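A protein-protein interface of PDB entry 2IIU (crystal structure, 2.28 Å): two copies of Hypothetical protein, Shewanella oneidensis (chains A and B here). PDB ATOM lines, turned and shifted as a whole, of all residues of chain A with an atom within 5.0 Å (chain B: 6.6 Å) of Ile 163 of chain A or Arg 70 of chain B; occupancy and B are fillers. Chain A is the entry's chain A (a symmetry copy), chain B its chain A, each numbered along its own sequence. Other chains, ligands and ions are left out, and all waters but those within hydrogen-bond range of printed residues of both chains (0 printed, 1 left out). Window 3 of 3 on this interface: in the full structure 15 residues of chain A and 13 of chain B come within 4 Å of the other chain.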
ATOM      1  N   VAL A 159      -2.323  -4.594 -18.769  1.00  0.00           N
ATOM      2  CA  VAL A 159      -3.162  -5.750 -18.539  1.00  0.00           C
ATOM      3  C   VAL A 159      -4.237  -5.428 -17.536  1.00  0.00           C
ATOM      4  O   VAL A 159      -5.388  -5.852 -17.707  1.00  0.00           O
ATOM      5  CB  VAL A 159      -2.318  -6.970 -18.082  1.00  0.00           C
ATOM      6  CG1 VAL A 159      -3.215  -8.108 -17.568  1.00  0.00           C
ATOM      7  CG2 VAL A 159      -1.447  -7.413 -19.228  1.00  0.00           C
ATOM      8  N   ALA A 160      -3.892  -4.705 -16.468  1.00  0.00           N
ATOM      9  CA  ALA A 160      -4.917  -4.305 -15.490  1.00  0.00           C
ATOM     10  C   ALA A 160      -6.071  -3.544 -16.160  1.00  0.00           C
ATOM     11  O   ALA A 160      -7.231  -3.771 -15.841  1.00  0.00           O
ATOM     12  CB  ALA A 160      -4.300  -3.444 -14.426  1.00  0.00           C
ATOM     13  N   LYS A 161      -5.726  -2.617 -17.051  1.00  0.00           N
ATOM     14  CA  LYS A 161      -6.703  -1.775 -17.752  1.00  0.00           C
ATOM     15  C   LYS A 161      -7.568  -2.616 -18.658  1.00  0.00           C
ATOM     16  O   LYS A 161      -8.790  -2.479 -18.700  1.00  0.00           O
ATOM     17  CB  LYS A 161      -6.002  -0.680 -18.592  1.00  0.00           C
ATOM     18  CG  LYS A 161      -5.317   0.457 -17.773  1.00  0.00           C
ATOM     19  CD  LYS A 161      -4.555   1.464 -18.686  1.00  0.00           C
ATOM     20  CE  LYS A 161      -3.777   2.566 -17.891  1.00  0.00           C
ATOM     21  N   MET A 162      -6.917  -3.500 -19.390  1.00  0.00           N
ATOM     22  CA  MET A 162      -7.609  -4.421 -20.301  1.00  0.00           C
ATOM     23  C   MET A 162      -8.638  -5.260 -19.547  1.00  0.00           C
ATOM     24  O   MET A 162      -9.766  -5.403 -19.978  1.00  0.00           O
ATOM     25  CB  MET A 162      -6.589  -5.330 -20.969  1.00  0.00           C
ATOM     26  CG  MET A 162      -7.127  -6.142 -22.098  1.00  0.00           C
ATOM     27  SD  MET A 162      -5.692  -7.223 -22.938  1.00  0.00           S
ATOM     28  CE  MET A 162      -5.706  -8.795 -21.639  1.00  0.00           C
ATOM     29  N   ILE A 163      -8.233  -5.813 -18.415  1.00  0.00           N
ATOM     30  CA  ILE A 163      -9.121  -6.570 -17.555  1.00  0.00           C
ATOM     31  C   ILE A 163     -10.296  -5.705 -17.101  1.00  0.00           C
ATOM     32  O   ILE A 163     -11.433  -6.125 -17.181  1.00  0.00           O
ATOM     33  CB  ILE A 163      -8.367  -7.093 -16.305  1.00  0.00           C
ATOM     34  CG1 ILE A 163      -7.364  -8.185 -16.690  1.00  0.00           C
ATOM     35  CG2 ILE A 163      -9.346  -7.696 -15.303  1.00  0.00           C
ATOM     36  CD1 ILE A 163      -6.558  -8.711 -15.473  1.00  0.00           C
ATOM     37  N   ASN A 164     -10.027  -4.486 -16.653  1.00  0.00           N
ATOM     38  CA  ASN A 164     -11.107  -3.612 -16.185  1.00  0.00           C
ATOM     39  C   ASN A 164     -12.105  -3.291 -17.305  1.00  0.00           C
ATOM     40  O   ASN A 164     -13.299  -3.282 -17.087  1.00  0.00           O
ATOM     41  CB  ASN A 164     -10.545  -2.314 -15.582  1.00  0.00           C
ATOM     42  CG  ASN A 164      -9.732  -2.556 -14.299  1.00  0.00           C
ATOM     43  OD1 ASN A 164     -10.001  -3.482 -13.558  1.00  0.00           O
ATOM     44  ND2 ASN A 164      -8.713  -1.730 -14.065  1.00  0.00           N
ATOM     45  N   GLU A 165     -11.591  -3.008 -18.493  1.00  0.00           N
ATOM     46  CA  GLU A 165     -12.419  -2.673 -19.647  1.00  0.00           C
ATOM     47  C   GLU A 165     -13.311  -3.855 -20.068  1.00  0.00           C
ATOM     48  O   GLU A 165     -14.507  -3.686 -20.354  1.00  0.00           O
ATOM     49  CB  GLU A 165     -11.520  -2.260 -20.824  1.00  0.00           C
ATOM     50  CG  GLU A 165     -10.878  -0.886 -20.729  1.00  0.00           C
ATOM     51  CD  GLU A 165     -11.748   0.217 -21.269  1.00  0.00           C
ATOM     52  N   LEU A 166     -12.736  -5.043 -20.067  1.00  0.00           N
ATOM     53  CA  LEU A 166     -13.492  -6.239 -20.394  1.00  0.00           C
ATOM     54  C   LEU A 166     -14.558  -6.572 -19.340  1.00  0.00           C
ATOM     55  O   LEU A 166     -15.671  -6.985 -19.689  1.00  0.00           O
ATOM     56  CB  LEU A 166     -12.545  -7.428 -20.581  1.00  0.00           C
ATOM     57  CG  LEU A 166     -13.215  -8.742 -21.014  1.00  0.00           C
ATOM     58  CD1 LEU A 166     -14.008  -8.628 -22.343  1.00  0.00           C
ATOM     59  CD2 LEU A 166     -12.195  -9.871 -21.098  1.00  0.00           C
ATOM     60  N   ASP A 167     -14.226  -6.412 -18.062  1.00  0.00           N
ATOM     61  CA  ASP A 167     -15.203  -6.678 -17.000  1.00  0.00           C
ATOM     62  C   ASP A 167     -16.454  -5.812 -17.158  1.00  0.00           C
ATOM     63  O   ASP A 167     -17.564  -6.264 -16.857  1.00  0.00           O
ATOM     64  CB  ASP A 167     -14.599  -6.451 -15.602  1.00  0.00           C
ATOM     65  CG  ASP A 167     -13.567  -7.517 -15.214  1.00  0.00           C
ATOM     66  OD1 ASP A 167     -13.358  -8.525 -15.972  1.00  0.00           O
ATOM     67  OD2 ASP A 167     -12.947  -7.318 -14.139  1.00  0.00           O
ATOM     68  N   GLU A 221      -1.871 -10.887 -23.767  1.00  0.00           N
ATOM     69  CA  GLU A 221      -1.391 -10.989 -22.404  1.00  0.00           C
ATOM     70  C   GLU A 221      -0.258 -12.020 -22.333  1.00  0.00           C
ATOM     71  O   GLU A 221       0.740 -11.781 -21.655  1.00  0.00           O
ATOM     72  CB  GLU A 221      -2.532 -11.269 -21.444  1.00  0.00           C
ATOM     73  CG  GLU A 221      -2.130 -11.535 -20.017  1.00  0.00           C
ATOM     74  CD  GLU A 221      -3.354 -11.743 -19.122  1.00  0.00           C
ATOM     75  OE1 GLU A 221      -4.459 -11.891 -19.669  1.00  0.00           O
ATOM     76  OE2 GLU A 221      -3.200 -11.711 -17.893  1.00  0.00           O
ATOM     77  N   ASP B  63     -12.446 -15.736  -9.933  1.00  0.00           N
ATOM     78  CA  ASP B  63     -12.053 -14.617 -10.741  1.00  0.00           C
ATOM     79  C   ASP B  63     -11.082 -13.679 -10.072  1.00  0.00           C
ATOM     80  O   ASP B  63     -10.142 -13.206 -10.717  1.00  0.00           O
ATOM     81  CB  ASP B  63     -13.252 -13.777 -11.071  1.00  0.00           C
ATOM     82  CG  ASP B  63     -13.584 -13.806 -12.478  1.00  0.00           C
ATOM     83  OD1 ASP B  63     -12.856 -13.098 -13.232  1.00  0.00           O
ATOM     84  OD2 ASP B  63     -14.594 -14.471 -12.809  1.00  0.00           O
ATOM     85  N   LEU B  65      -9.007 -14.383  -7.641  1.00  0.00           N
ATOM     86  CA  LEU B  65      -7.705 -15.066  -7.565  1.00  0.00           C
ATOM     87  C   LEU B  65      -7.019 -15.038  -8.920  1.00  0.00           C
ATOM     88  O   LEU B  65      -5.826 -14.867  -9.014  1.00  0.00           O
ATOM     89  CB  LEU B  65      -7.854 -16.536  -7.165  1.00  0.00           C
ATOM     90  CG  LEU B  65      -8.451 -16.854  -5.798  1.00  0.00           C
ATOM     91  CD1 LEU B  65      -8.679 -18.354  -5.620  1.00  0.00           C
ATOM     92  CD2 LEU B  65      -7.578 -16.321  -4.692  1.00  0.00           C
ATOM     93  N   LYS B  66      -7.795 -15.249  -9.968  1.00  0.00           N
ATOM     94  CA  LYS B  66      -7.283 -15.234 -11.361  1.00  0.00           C
ATOM     95  C   LYS B  66      -6.653 -13.869 -11.666  1.00  0.00           C
ATOM     96  O   LYS B  66      -5.525 -13.759 -12.145  1.00  0.00           O
ATOM     97  CB  LYS B  66      -8.442 -15.529 -12.321  1.00  0.00           C
ATOM     98  CG  LYS B  66      -8.116 -15.512 -13.815  1.00  0.00           C
ATOM     99  CD  LYS B  66      -9.455 -15.471 -14.609  1.00  0.00           C
ATOM    100  CE  LYS B  66      -9.260 -15.550 -16.115  1.00  0.00           C
ATOM    101  NZ  LYS B  66     -10.568 -15.337 -16.853  1.00  0.00           N
ATOM    102  N   ARG B  67      -7.367 -12.820 -11.335  1.00  0.00           N
ATOM    103  CA  ARG B  67      -6.891 -11.479 -11.550  1.00  0.00           C
ATOM    104  C   ARG B  67      -5.552 -11.217 -10.844  1.00  0.00           C
ATOM    105  O   ARG B  67      -4.619 -10.681 -11.445  1.00  0.00           O
ATOM    106  CB  ARG B  67      -7.943 -10.499 -11.042  1.00  0.00           C
ATOM    107  CG  ARG B  67      -7.579  -9.069 -11.278  1.00  0.00           C
ATOM    108  CD  ARG B  67      -8.456  -8.125 -10.486  1.00  0.00           C
ATOM    109  NE  ARG B  67      -7.941  -6.779 -10.676  1.00  0.00           N
ATOM    110  CZ  ARG B  67      -8.305  -5.931 -11.630  1.00  0.00           C
ATOM    111  NH1 ARG B  67      -9.239  -6.249 -12.520  1.00  0.00           N
ATOM    112  NH2 ARG B  67      -7.728  -4.741 -11.679  1.00  0.00           N
ATOM    113  N   GLU B  68      -5.465 -11.564  -9.559  1.00  0.00           N
ATOM    114  CA  GLU B  68      -4.250 -11.281  -8.785  1.00  0.00           C
ATOM    115  C   GLU B  68      -3.065 -12.034  -9.401  1.00  0.00           C
ATOM    116  O   GLU B  68      -1.986 -11.486  -9.544  1.00  0.00           O
ATOM    117  CB  GLU B  68      -4.441 -11.645  -7.300  1.00  0.00           C
ATOM    118  N   ILE B  69      -3.282 -13.286  -9.773  1.00  0.00           N
ATOM    119  CA  ILE B  69      -2.238 -14.072 -10.452  1.00  0.00           C
ATOM    120  C   ILE B  69      -1.804 -13.407 -11.745  1.00  0.00           C
ATOM    121  O   ILE B  69      -0.591 -13.207 -11.975  1.00  0.00           O
ATOM    122  CB  ILE B  69      -2.677 -15.517 -10.767  1.00  0.00           C
ATOM    123  CG1 ILE B  69      -2.808 -16.296  -9.456  1.00  0.00           C
ATOM    124  CG2 ILE B  69      -1.623 -16.180 -11.687  1.00  0.00           C
ATOM    125  CD1 ILE B  69      -3.554 -17.663  -9.538  1.00  0.00           C
ATOM    126  N   ARG B  70      -2.757 -13.001 -12.565  1.00  0.00           N
ATOM    127  CA  ARG B  70      -2.400 -12.349 -13.833  1.00  0.00           C
ATOM    128  C   ARG B  70      -1.624 -11.071 -13.670  1.00  0.00           C
ATOM    129  O   ARG B  70      -0.850 -10.721 -14.533  1.00  0.00           O
ATOM    130  CB  ARG B  70      -3.613 -12.064 -14.673  1.00  0.00           C
ATOM    131  CG  ARG B  70      -4.263 -13.324 -15.131  1.00  0.00           C
ATOM    132  CD  ARG B  70      -5.726 -13.083 -15.460  1.00  0.00           C
ATOM    133  NE  ARG B  70      -5.896 -12.352 -16.711  1.00  0.00           N
ATOM    134  CZ  ARG B  70      -7.080 -11.956 -17.181  1.00  0.00           C
ATOM    135  NH1 ARG B  70      -8.195 -12.109 -16.475  1.00  0.00           N
ATOM    136  NH2 ARG B  70      -7.144 -11.353 -18.352  1.00  0.00           N
ATOM    137  N   LEU B  71      -1.843 -10.358 -12.583  1.00  0.00           N
ATOM    138  CA  LEU B  71      -1.151  -9.136 -12.378  1.00  0.00           C
ATOM    139  C   LEU B  71       0.119  -9.292 -11.530  1.00  0.00           C
ATOM    140  O   LEU B  71       0.780  -8.315 -11.307  1.00  0.00           O
ATOM    141  CB  LEU B  71      -2.083  -8.101 -11.727  1.00  0.00           C
ATOM    142  CG  LEU B  71      -3.333  -7.673 -12.499  1.00  0.00           C
ATOM    143  CD1 LEU B  71      -4.113  -6.655 -11.676  1.00  0.00           C
ATOM    144  CD2 LEU B  71      -2.932  -7.097 -13.888  1.00  0.00           C
ATOM    145  N   THR B  72       0.468 -10.496 -11.073  1.00  0.00           N
ATOM    146  CA  THR B  72       1.646 -10.693 -10.205  1.00  0.00           C
ATOM    147  C   THR B  72       2.615 -11.804 -10.622  1.00  0.00           C
ATOM    148  O   THR B  72       2.511 -12.422 -11.702  1.00  0.00           O
ATOM    149  CB  THR B  72       1.197 -11.004  -8.732  1.00  0.00           C
ATOM    150  OG1 THR B  72       0.393 -12.194  -8.708  1.00  0.00           O
ATOM    151  CG2 THR B  72       0.374  -9.852  -8.130  1.00  0.00           C
ATOM    152  N   LEU B  87      -0.234 -19.089 -17.039  1.00  0.00           N
ATOM    153  CA  LEU B  87      -1.385 -18.321 -17.528  1.00  0.00           C
ATOM    154  C   LEU B  87      -2.353 -19.199 -18.336  1.00  0.00           C
ATOM    155  O   LEU B  87      -3.561 -19.148 -18.125  1.00  0.00           O
ATOM    156  CB  LEU B  87      -0.923 -17.119 -18.379  1.00  0.00           C
ATOM    157  CG  LEU B  87      -0.248 -15.985 -17.610  1.00  0.00           C
ATOM    158  CD1 LEU B  87       0.211 -14.908 -18.578  1.00  0.00           C
ATOM    159  CD2 LEU B  87      -1.198 -15.405 -16.562  1.00  0.00           C
ATOM    160  N   LEU B  90      -4.206 -21.434 -15.941  1.00  0.00           N
ATOM    161  CA  LEU B  90      -5.239 -20.633 -15.269  1.00  0.00           C
ATOM    162  C   LEU B  90      -6.456 -20.411 -16.129  1.00  0.00           C
ATOM    163  O   LEU B  90      -7.583 -20.432 -15.667  1.00  0.00           O
ATOM    164  CB  LEU B  90      -4.632 -19.255 -14.914  1.00  0.00           C
ATOM    165  CG  LEU B  90      -5.436 -18.288 -14.070  1.00  0.00           C
ATOM    166  CD1 LEU B  90      -5.747 -18.887 -12.743  1.00  0.00           C
ATOM    167  CD2 LEU B  90      -4.614 -16.998 -13.907  1.00  0.00           C
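Val 159 of chain A touches Leu 71 of chain B (CG1 to CD2, 3.8 Å). CD2 of Leu 71 of chain B touches N of Ala 160 of chain A, at 3.6 Å. CG2 of Ile 163 of chain A touches NH1 of Arg 67 of chain B, at 3.1 Å. Ile 163 of chain A touches Arg 70 of chain B.
Hydrophobic or aromatic side chains of chain A that line the printed part of chain B: Val 159, Ala 160 and Ile 163. Of the 11 printed residues of chain B, 3 touch a printed residue of chain A. Among the printed residues, 6 pairs touch across the chains. Among the printed residues, Asp or Glu carboxylates within 4 Å of a Lys or Arg side-chain nitrogen of the other chain: Glu 221 of chain A with Arg 70 of chain B (3.0 Å).
No position is printed for both chains. Of the 6 pairs that touch across the chains among the printed residues, none has its exchanged pair printed and touching as well.
Ile 163 of chain A touches just these residues of chain B: Arg 67 (3.1 Å) and Arg 70 (3.6 Å). Arg 70 of chain B touches just these residues of chain A: Ile 163 and Glu 221. Of the printed residues of chain B, Asn 164 of chain A touches Arg 67. Printed residues of chain B within 4 Å of Ala 160 of chain A: Leu 71 (3.6 Å). Of the printed residues of chain A, Arg 67 of chain B touches Ile 163 (3.1 Å) and Asn 164 (3.1 Å). The nearest printed residue of chain B that does not touch Glu 221 of chain A is Leu 87 of chain B (4.4 Å).
The backbone carbonyl oxygen of Ala 160 of chain A is in hydrogen-bond range of the side-chain amide nitrogen of Asn 164 of chain A (3.1 Å).
The guanidinium group (NE) of Arg 70 of chain B is in salt-bridge range of the side-chain carboxylate (OE2) of Glu 221 of chain A, at 3.0 Å. The guanidinium group (NH1) of Arg 67 of chain B lies within hydrogen-bond range of the side-chain amide oxygen (OD1) of Asn 164 of chain A, 3.1 Å away.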
